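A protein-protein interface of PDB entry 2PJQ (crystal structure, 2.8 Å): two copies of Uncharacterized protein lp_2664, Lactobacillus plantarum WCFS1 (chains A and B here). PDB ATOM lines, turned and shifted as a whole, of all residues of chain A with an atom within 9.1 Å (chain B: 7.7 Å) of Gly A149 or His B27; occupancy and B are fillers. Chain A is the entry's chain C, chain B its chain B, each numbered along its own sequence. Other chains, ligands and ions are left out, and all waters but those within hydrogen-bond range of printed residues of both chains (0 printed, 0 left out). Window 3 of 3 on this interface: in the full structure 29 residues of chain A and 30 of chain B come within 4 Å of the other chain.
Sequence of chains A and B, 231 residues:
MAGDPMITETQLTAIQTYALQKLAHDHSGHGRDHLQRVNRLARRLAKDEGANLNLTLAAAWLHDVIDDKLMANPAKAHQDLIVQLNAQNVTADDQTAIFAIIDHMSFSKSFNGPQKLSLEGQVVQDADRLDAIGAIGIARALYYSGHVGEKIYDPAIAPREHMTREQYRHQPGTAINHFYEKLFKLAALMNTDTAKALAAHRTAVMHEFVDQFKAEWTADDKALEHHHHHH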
ATOM      1  N   LEU A 142      -3.810 -10.202   9.119  1.00  0.00           N
ATOM      2  CA  LEU A 142      -4.423 -11.202   9.991  1.00  0.00           C
ATOM      3  C   LEU A 142      -4.742 -10.749  11.394  1.00  0.00           C
ATOM      4  O   LEU A 142      -5.709 -11.213  11.994  1.00  0.00           O
ATOM      5  CB  LEU A 142      -3.546 -12.448  10.062  1.00  0.00           C
ATOM      6  CG  LEU A 142      -3.716 -13.342   8.833  1.00  0.00           C
ATOM      7  CD1 LEU A 142      -2.396 -13.450   8.110  1.00  0.00           C
ATOM      8  CD2 LEU A 142      -4.243 -14.707   9.253  1.00  0.00           C
ATOM      9  N   TYR A 143      -3.915  -9.872  11.936  1.00  0.00           N
ATOM     10  CA  TYR A 143      -4.175  -9.363  13.262  1.00  0.00           C
ATOM     11  C   TYR A 143      -5.621  -8.853  13.156  1.00  0.00           C
ATOM     12  O   TYR A 143      -6.529  -9.319  13.878  1.00  0.00           O
ATOM     13  CB  TYR A 143      -3.190  -8.236  13.565  1.00  0.00           C
ATOM     14  CG  TYR A 143      -3.327  -7.600  14.929  1.00  0.00           C
ATOM     15  CD1 TYR A 143      -4.327  -6.661  15.193  1.00  0.00           C
ATOM     16  CD2 TYR A 143      -2.420  -7.897  15.943  1.00  0.00           C
ATOM     17  CE1 TYR A 143      -4.407  -6.027  16.426  1.00  0.00           C
ATOM     18  CE2 TYR A 143      -2.494  -7.277  17.174  1.00  0.00           C
ATOM     19  CZ  TYR A 143      -3.480  -6.341  17.407  1.00  0.00           C
ATOM     20  OH  TYR A 143      -3.494  -5.688  18.607  1.00  0.00           O
ATOM     21  N   TYR A 144      -5.831  -7.933  12.216  1.00  0.00           N
ATOM     22  CA  TYR A 144      -7.153  -7.370  11.960  1.00  0.00           C
ATOM     23  C   TYR A 144      -8.231  -8.430  11.841  1.00  0.00           C
ATOM     24  O   TYR A 144      -9.299  -8.278  12.420  1.00  0.00           O
ATOM     25  CB  TYR A 144      -7.190  -6.578  10.659  1.00  0.00           C
ATOM     26  CG  TYR A 144      -8.565  -6.010  10.408  1.00  0.00           C
ATOM     27  CD1 TYR A 144      -8.999  -4.882  11.104  1.00  0.00           C
ATOM     28  CD2 TYR A 144      -9.455  -6.624   9.523  1.00  0.00           C
ATOM     29  CE1 TYR A 144     -10.272  -4.379  10.931  1.00  0.00           C
ATOM     30  CE2 TYR A 144     -10.742  -6.126   9.345  1.00  0.00           C
ATOM     31  CZ  TYR A 144     -11.141  -5.001  10.053  1.00  0.00           C
ATOM     32  OH  TYR A 144     -12.402  -4.478   9.897  1.00  0.00           O
ATOM     33  N   SER A 145      -7.976  -9.472  11.050  1.00  0.00           N
ATOM     34  CA  SER A 145      -8.953 -10.550  10.871  1.00  0.00           C
ATOM     35  C   SER A 145      -9.262 -11.199  12.220  1.00  0.00           C
ATOM     36  O   SER A 145     -10.429 -11.430  12.557  1.00  0.00           O
ATOM     37  CB  SER A 145      -8.425 -11.613   9.902  1.00  0.00           C
ATOM     38  OG  SER A 145      -8.319 -11.114   8.575  1.00  0.00           O
ATOM     39  N   GLY A 146      -8.209 -11.488  12.984  1.00  0.00           N
ATOM     40  CA  GLY A 146      -8.382 -12.090  14.287  1.00  0.00           C
ATOM     41  C   GLY A 146      -9.104 -11.156  15.241  1.00  0.00           C
ATOM     42  O   GLY A 146      -9.663 -11.598  16.238  1.00  0.00           O
ATOM     43  N   HIS A 147      -9.082  -9.861  14.955  1.00  0.00           N
ATOM     44  CA  HIS A 147      -9.773  -8.887  15.796  1.00  0.00           C
ATOM     45  C   HIS A 147     -11.235  -8.839  15.368  1.00  0.00           C
ATOM     46  O   HIS A 147     -12.055  -8.152  15.982  1.00  0.00           O
ATOM     47  CB  HIS A 147      -9.146  -7.500  15.626  1.00  0.00           C
ATOM     48  CG  HIS A 147     -10.024  -6.365  16.062  1.00  0.00           C
ATOM     49  ND1 HIS A 147     -10.457  -6.207  17.363  1.00  0.00           N
ATOM     50  CD2 HIS A 147     -10.507  -5.303  15.376  1.00  0.00           C
ATOM     51  CE1 HIS A 147     -11.162  -5.093  17.458  1.00  0.00           C
ATOM     52  NE2 HIS A 147     -11.206  -4.525  16.266  1.00  0.00           N
ATOM     53  N   VAL A 148     -11.557  -9.584  14.315  1.00  0.00           N
ATOM     54  CA  VAL A 148     -12.914  -9.598  13.789  1.00  0.00           C
ATOM     55  C   VAL A 148     -13.515 -11.011  13.696  1.00  0.00           C
ATOM     56  O   VAL A 148     -14.688 -11.164  13.353  1.00  0.00           O
ATOM     57  CB  VAL A 148     -12.965  -8.901  12.385  1.00  0.00           C
ATOM     58  CG1 VAL A 148     -14.370  -8.850  11.879  1.00  0.00           C
ATOM     59  CG2 VAL A 148     -12.429  -7.489  12.473  1.00  0.00           C
ATOM     60  N   GLY A 149     -12.735 -12.046  14.012  1.00  0.00           N
ATOM     61  CA  GLY A 149     -13.278 -13.398  13.939  1.00  0.00           C
ATOM     62  C   GLY A 149     -13.701 -13.753  12.523  1.00  0.00           C
ATOM     63  O   GLY A 149     -14.694 -14.446  12.272  1.00  0.00           O
ATOM     64  N   GLU A 150     -12.899 -13.264  11.590  1.00  0.00           N
ATOM     65  CA  GLU A 150     -13.090 -13.449  10.164  1.00  0.00           C
ATOM     66  C   GLU A 150     -12.430 -14.763   9.738  1.00  0.00           C
ATOM     67  O   GLU A 150     -11.283 -15.025  10.095  1.00  0.00           O
ATOM     68  CB  GLU A 150     -12.422 -12.274   9.485  1.00  0.00           C
ATOM     69  CG  GLU A 150     -12.579 -12.164   8.015  1.00  0.00           C
ATOM     70  CD  GLU A 150     -11.752 -11.015   7.496  1.00  0.00           C
ATOM     71  OE1 GLU A 150     -10.525 -11.204   7.338  1.00  0.00           O
ATOM     72  OE2 GLU A 150     -12.331  -9.923   7.281  1.00  0.00           O
ATOM     73  N   LYS A 151     -13.127 -15.590   8.969  1.00  0.00           N
ATOM     74  CA  LYS A 151     -12.519 -16.847   8.570  1.00  0.00           C
ATOM     75  C   LYS A 151     -11.196 -16.628   7.833  1.00  0.00           C
ATOM     76  O   LYS A 151     -11.136 -15.997   6.763  1.00  0.00           O
ATOM     77  CB  LYS A 151     -13.462 -17.681   7.712  1.00  0.00           C
ATOM     78  CG  LYS A 151     -12.964 -19.106   7.591  1.00  0.00           C
ATOM     79  CD  LYS A 151     -13.870 -19.961   6.728  1.00  0.00           C
ATOM     80  CE  LYS A 151     -15.281 -20.057   7.303  1.00  0.00           C
ATOM     81  NZ  LYS A 151     -16.183 -20.780   6.369  1.00  0.00           N
ATOM     82  N   ILE A 152     -10.135 -17.162   8.430  1.00  0.00           N
ATOM     83  CA  ILE A 152      -8.802 -17.040   7.883  1.00  0.00           C
ATOM     84  C   ILE A 152      -8.702 -17.596   6.484  1.00  0.00           C
ATOM     85  O   ILE A 152      -8.075 -16.991   5.611  1.00  0.00           O
ATOM     86  CB  ILE A 152      -7.779 -17.763   8.745  1.00  0.00           C
ATOM     87  CG1 ILE A 152      -7.720 -17.108  10.123  1.00  0.00           C
ATOM     88  CG2 ILE A 152      -6.428 -17.724   8.071  1.00  0.00           C
ATOM     89  CD1 ILE A 152      -6.644 -17.664  11.044  1.00  0.00           C
ATOM     90  N   PRO A 172     -18.291 -10.455   3.841  1.00  0.00           N
ATOM     91  CA  PRO A 172     -17.088 -11.022   4.455  1.00  0.00           C
ATOM     92  C   PRO A 172     -16.383 -12.084   3.619  1.00  0.00           C
ATOM     93  O   PRO A 172     -17.025 -13.008   3.122  1.00  0.00           O
ATOM     94  CB  PRO A 172     -17.614 -11.621   5.760  1.00  0.00           C
ATOM     95  CG  PRO A 172     -19.006 -11.012   5.930  1.00  0.00           C
ATOM     96  CD  PRO A 172     -19.495 -10.936   4.534  1.00  0.00           C
ATOM     97  N   GLY A 173     -15.063 -11.961   3.485  1.00  0.00           N
ATOM     98  CA  GLY A 173     -14.281 -12.948   2.749  1.00  0.00           C
ATOM     99  C   GLY A 173     -13.314 -13.645   3.704  1.00  0.00           C
ATOM    100  O   GLY A 173     -13.552 -13.705   4.908  1.00  0.00           O
ATOM    101  N   THR A 174     -12.219 -14.181   3.190  1.00  0.00           N
ATOM    102  CA  THR A 174     -11.265 -14.834   4.076  1.00  0.00           C
ATOM    103  C   THR A 174      -9.984 -14.013   4.116  1.00  0.00           C
ATOM    104  O   THR A 174      -9.607 -13.401   3.119  1.00  0.00           O
ATOM    105  CB  THR A 174     -10.943 -16.241   3.597  1.00  0.00           C
ATOM    106  OG1 THR A 174     -10.063 -16.173   2.471  1.00  0.00           O
ATOM    107  CG2 THR A 174     -12.209 -16.938   3.164  1.00  0.00           C
ATOM    108  N   ALA A 175      -9.328 -13.991   5.272  1.00  0.00           N
ATOM    109  CA  ALA A 175      -8.103 -13.229   5.423  1.00  0.00           C
ATOM    110  C   ALA A 175      -7.142 -13.620   4.301  1.00  0.00           C
ATOM    111  O   ALA A 175      -6.519 -12.762   3.666  1.00  0.00           O
ATOM    112  CB  ALA A 175      -7.484 -13.494   6.780  1.00  0.00           C
ATOM    113  N   LEU B  23     -16.196 -25.588  20.514  1.00  0.00           N
ATOM    114  CA  LEU B  23     -15.284 -24.655  19.857  1.00  0.00           C
ATOM    115  C   LEU B  23     -15.903 -23.894  18.711  1.00  0.00           C
ATOM    116  O   LEU B  23     -15.199 -23.324  17.894  1.00  0.00           O
ATOM    117  CB  LEU B  23     -14.019 -25.367  19.384  1.00  0.00           C
ATOM    118  CG  LEU B  23     -13.128 -25.730  20.565  1.00  0.00           C
ATOM    119  CD1 LEU B  23     -11.933 -26.510  20.069  1.00  0.00           C
ATOM    120  CD2 LEU B  23     -12.698 -24.473  21.296  1.00  0.00           C
ATOM    121  N   ALA B  24     -17.225 -23.901  18.648  1.00  0.00           N
ATOM    122  CA  ALA B  24     -17.922 -23.155  17.618  1.00  0.00           C
ATOM    123  C   ALA B  24     -17.856 -21.701  18.101  1.00  0.00           C
ATOM    124  O   ALA B  24     -17.849 -21.436  19.311  1.00  0.00           O
ATOM    125  CB  ALA B  24     -19.364 -23.623  17.518  1.00  0.00           C
ATOM    126  N   HIS B  25     -17.798 -20.758  17.171  1.00  0.00           N
ATOM    127  CA  HIS B  25     -17.714 -19.352  17.552  1.00  0.00           C
ATOM    128  C   HIS B  25     -16.401 -19.148  18.315  1.00  0.00           C
ATOM    129  O   HIS B  25     -16.354 -18.394  19.284  1.00  0.00           O
ATOM    130  CB  HIS B  25     -18.891 -18.974  18.466  1.00  0.00           C
ATOM    131  CG  HIS B  25     -20.170 -19.677  18.129  1.00  0.00           C
ATOM    132  ND1 HIS B  25     -20.857 -19.459  16.952  1.00  0.00           N
ATOM    133  CD2 HIS B  25     -20.855 -20.642  18.790  1.00  0.00           C
ATOM    134  CE1 HIS B  25     -21.906 -20.263  16.901  1.00  0.00           C
ATOM    135  NE2 HIS B  25     -21.925 -20.991  18.005  1.00  0.00           N
ATOM    136  N   ASP B  26     -15.337 -19.826  17.892  1.00  0.00           N
ATOM    137  CA  ASP B  26     -14.058 -19.684  18.573  1.00  0.00           C
ATOM    138  C   ASP B  26     -13.452 -18.302  18.346  1.00  0.00           C
ATOM    139  O   ASP B  26     -13.271 -17.539  19.292  1.00  0.00           O
ATOM    140  CB  ASP B  26     -13.072 -20.743  18.096  1.00  0.00           C
ATOM    141  CG  ASP B  26     -11.658 -20.479  18.588  1.00  0.00           C
ATOM    142  OD1 ASP B  26     -11.407 -20.640  19.801  1.00  0.00           O
ATOM    143  OD2 ASP B  26     -10.801 -20.093  17.761  1.00  0.00           O
ATOM    144  N   HIS B  27     -13.125 -17.987  17.096  1.00  0.00           N
ATOM    145  CA  HIS B  27     -12.539 -16.685  16.734  1.00  0.00           C
ATOM    146  C   HIS B  27     -11.197 -16.329  17.377  1.00  0.00           C
ATOM    147  O   HIS B  27     -10.902 -15.152  17.577  1.00  0.00           O
ATOM    148  CB  HIS B  27     -13.548 -15.571  17.012  1.00  0.00           C
ATOM    149  CG  HIS B  27     -14.907 -15.875  16.481  1.00  0.00           C
ATOM    150  ND1 HIS B  27     -15.121 -16.247  15.171  1.00  0.00           N
ATOM    151  CD2 HIS B  27     -16.107 -15.973  17.099  1.00  0.00           C
ATOM    152  CE1 HIS B  27     -16.389 -16.568  15.006  1.00  0.00           C
ATOM    153  NE2 HIS B  27     -17.011 -16.411  16.163  1.00  0.00           N
ATOM    154  N   SER B  28     -10.395 -17.345  17.700  1.00  0.00           N
ATOM    155  CA  SER B  28      -9.081 -17.127  18.309  1.00  0.00           C
ATOM    156  C   SER B  28      -8.028 -17.952  17.582  1.00  0.00           C
ATOM    157  O   SER B  28      -6.833 -17.811  17.842  1.00  0.00           O
ATOM    158  CB  SER B  28      -9.087 -17.518  19.784  1.00  0.00           C
ATOM    159  OG  SER B  28      -9.260 -18.911  19.939  1.00  0.00           O
ATOM    160  N   GLY B  29      -8.487 -18.805  16.669  1.00  0.00           N
ATOM    161  CA  GLY B  29      -7.583 -19.647  15.916  1.00  0.00           C
ATOM    162  C   GLY B  29      -7.548 -21.037  16.518  1.00  0.00           C
ATOM    163  O   GLY B  29      -6.508 -21.702  16.568  1.00  0.00           O
ATOM    164  N   HIS B  30      -8.696 -21.490  16.989  1.00  0.00           N
ATOM    165  CA  HIS B  30      -8.773 -22.802  17.607  1.00  0.00           C
ATOM    166  C   HIS B  30     -10.147 -23.402  17.334  1.00  0.00           C
ATOM    167  O   HIS B  30     -10.704 -24.124  18.163  1.00  0.00           O
ATOM    168  CB  HIS B  30      -8.534 -22.671  19.117  1.00  0.00           C
ATOM    169  CG  HIS B  30      -7.235 -22.010  19.465  1.00  0.00           C
ATOM    170  ND1 HIS B  30      -6.074 -22.717  19.694  1.00  0.00           N
ATOM    171  CD2 HIS B  30      -6.904 -20.703  19.567  1.00  0.00           C
ATOM    172  CE1 HIS B  30      -5.084 -21.874  19.918  1.00  0.00           C
ATOM    173  NE2 HIS B  30      -5.560 -20.645  19.846  1.00  0.00           N
ATOM    174  N   GLY B  31     -10.679 -23.092  16.157  1.00  0.00           N
ATOM    175  CA  GLY B  31     -11.982 -23.586  15.769  1.00  0.00           C
ATOM    176  C   GLY B  31     -11.868 -24.902  15.039  1.00  0.00           C
ATOM    177  O   GLY B  31     -10.841 -25.569  15.108  1.00  0.00           O
ATOM    178  N   TYR B 143      -3.268 -13.928  14.312  1.00  0.00           N
ATOM    179  CA  TYR B 143      -4.725 -13.912  14.304  1.00  0.00           C
ATOM    180  C   TYR B 143      -5.230 -13.946  15.737  1.00  0.00           C
ATOM    181  O   TYR B 143      -6.326 -13.479  16.041  1.00  0.00           O
ATOM    182  CB  TYR B 143      -5.241 -15.104  13.521  1.00  0.00           C
ATOM    183  CG  TYR B 143      -6.726 -15.224  13.508  1.00  0.00           C
ATOM    184  CD1 TYR B 143      -7.410 -15.819  14.572  1.00  0.00           C
ATOM    185  CD2 TYR B 143      -7.466 -14.768  12.420  1.00  0.00           C
ATOM    186  CE1 TYR B 143      -8.802 -15.965  14.547  1.00  0.00           C
ATOM    187  CE2 TYR B 143      -8.855 -14.909  12.384  1.00  0.00           C
ATOM    188  CZ  TYR B 143      -9.512 -15.510  13.446  1.00  0.00           C
ATOM    189  OH  TYR B 143     -10.869 -15.680  13.385  1.00  0.00           O
ATOM    190  N   TYR B 144      -4.413 -14.504  16.622  1.00  0.00           N
ATOM    191  CA  TYR B 144      -4.746 -14.583  18.031  1.00  0.00           C
ATOM    192  C   TYR B 144      -4.523 -13.218  18.692  1.00  0.00           C
ATOM    193  O   TYR B 144      -5.310 -12.781  19.540  1.00  0.00           O
ATOM    194  CB  TYR B 144      -3.871 -15.626  18.707  1.00  0.00           C
ATOM    195  CG  TYR B 144      -4.084 -15.706  20.199  1.00  0.00           C
ATOM    196  CD1 TYR B 144      -5.254 -16.241  20.728  1.00  0.00           C
ATOM    197  CD2 TYR B 144      -3.127 -15.219  21.077  1.00  0.00           C
ATOM    198  CE1 TYR B 144      -5.451 -16.281  22.092  1.00  0.00           C
ATOM    199  CE2 TYR B 144      -3.318 -15.255  22.426  1.00  0.00           C
ATOM    200  CZ  TYR B 144      -4.470 -15.781  22.935  1.00  0.00           C
ATOM    201  OH  TYR B 144      -4.649 -15.803  24.296  1.00  0.00           O
ATOM    202  N   GLY B 146      -4.760 -10.404  17.279  1.00  0.00           N
ATOM    203  CA  GLY B 146      -5.824  -9.508  16.875  1.00  0.00           C
ATOM    204  C   GLY B 146      -6.957  -9.734  17.858  1.00  0.00           C
ATOM    205  O   GLY B 146      -7.462  -8.812  18.520  1.00  0.00           O
ATOM    206  N   HIS B 147      -7.333 -10.999  17.961  1.00  0.00           N
ATOM    207  CA  HIS B 147      -8.393 -11.416  18.853  1.00  0.00           C
ATOM    208  C   HIS B 147      -8.239 -10.879  20.283  1.00  0.00           C
ATOM    209  O   HIS B 147      -9.173 -10.314  20.850  1.00  0.00           O
ATOM    210  CB  HIS B 147      -8.446 -12.944  18.876  1.00  0.00           C
ATOM    211  CG  HIS B 147      -9.394 -13.505  19.887  1.00  0.00           C
ATOM    212  ND1 HIS B 147     -10.745 -13.244  19.864  1.00  0.00           N
ATOM    213  CD2 HIS B 147      -9.184 -14.306  20.958  1.00  0.00           C
ATOM    214  CE1 HIS B 147     -11.328 -13.860  20.877  1.00  0.00           C
ATOM    215  NE2 HIS B 147     -10.402 -14.511  21.558  1.00  0.00           N
ATOM    216  N   VAL B 148      -7.061 -11.036  20.859  1.00  0.00           N
ATOM    217  CA  VAL B 148      -6.852 -10.611  22.231  1.00  0.00           C
ATOM    218  C   VAL B 148      -6.490  -9.139  22.404  1.00  0.00           C
ATOM    219  O   VAL B 148      -6.651  -8.588  23.486  1.00  0.00           O
ATOM    220  CB  VAL B 148      -5.767 -11.510  22.907  1.00  0.00           C
ATOM    221  CG1 VAL B 148      -5.233 -10.860  24.177  1.00  0.00           C
ATOM    222  CG2 VAL B 148      -6.356 -12.865  23.224  1.00  0.00           C
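Tyr A143 touches Gly B146, and with the chains exchanged Gly A146 touches Tyr B143. Gly A146 touches its own counterpart, Gly B146. Gly A146 touches His B147, and with the chains exchanged His A147 touches Gly B146. His B147 touches its own counterpart, His A147.
Hydrophobic or aromatic side chains of chain A that line the printed part of chain B: Tyr A143, His A147 and Ile A152. Printed residues of chain B that touch a printed residue of chain A: His B27, Tyr B143, Gly B146 and His B147. Among the printed residues, 13 pairs touch across the chains. Among the printed residues, no Asp or Glu carboxylate lies within 4 Å of a Lys or Arg side-chain nitrogen of the other chain.
Among the printed residues, merely in contact across the chains: Gly A146 with Tyr B143 (3.0 Å), Tyr A143 with Gly B146 (3.1 Å), Ile A152 with Tyr B143 (3.3 Å), Gly A149 with Tyr B143 (3.4 Å), His A147 with Gly B146 (3.6 Å), His A147 with His B147 (3.7 Å), Gly A146 with Gly B146 (3.7 Å), Leu A142 with Tyr B143 (3.7 Å), Ser A145 with Tyr B143 (3.7 Å) and Gly A146 with His B27 (3.99 Å).
O of His B27 sits at hydrogen-bond distance from ND1 of His B147. The side-chain hydroxyl of Ser A145 sits at hydrogen-bond distance from the side-chain carboxylate of Glu A150, at 2.5 Å. The backbone carbonyl oxygen of Ile A152 sits at hydrogen-bond distance from the backbone NH of Ala A175 (3.3 Å).
Gly A149 touches just these residues of chain B: His B27 and Tyr B143. No residue of chain A comes within 4 Å of Asp B26. Ser B28 touches none of the printed residues of chain A. Of the printed residues of chain B, His A147 touches Gly B146 (3.6 Å) and His B147 (3.7 Å). Of the printed residues of chain B, Ser A145 touches Tyr B143 (3.7 Å). Printed residues of chain A within 4 Å of Tyr B143: Leu A142 (3.7 Å), Ser A145 (3.7 Å), Gly A146 (3.0 Å), Gly A149 (3.4 Å), Glu A150 (3.3 Å) and Ile A152 (3.3 Å). Of the printed residues of chain B, Leu A142 touches Tyr B143. Of the printed residues of chain B, Gly A146 touches His B27, Tyr B143, Gly B146 and His B147.
The backbone carbonyl oxygen (O) of Glu A150 sits close to the side-chain hydroxyl (OH) of Tyr B143, at 3.4 Å. O of Gly A149 is in hydrogen-bond range of ND1 of His B27 (3.4 Å). N of His B147 lies close to O of Gly A146, 3.0 Å away.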
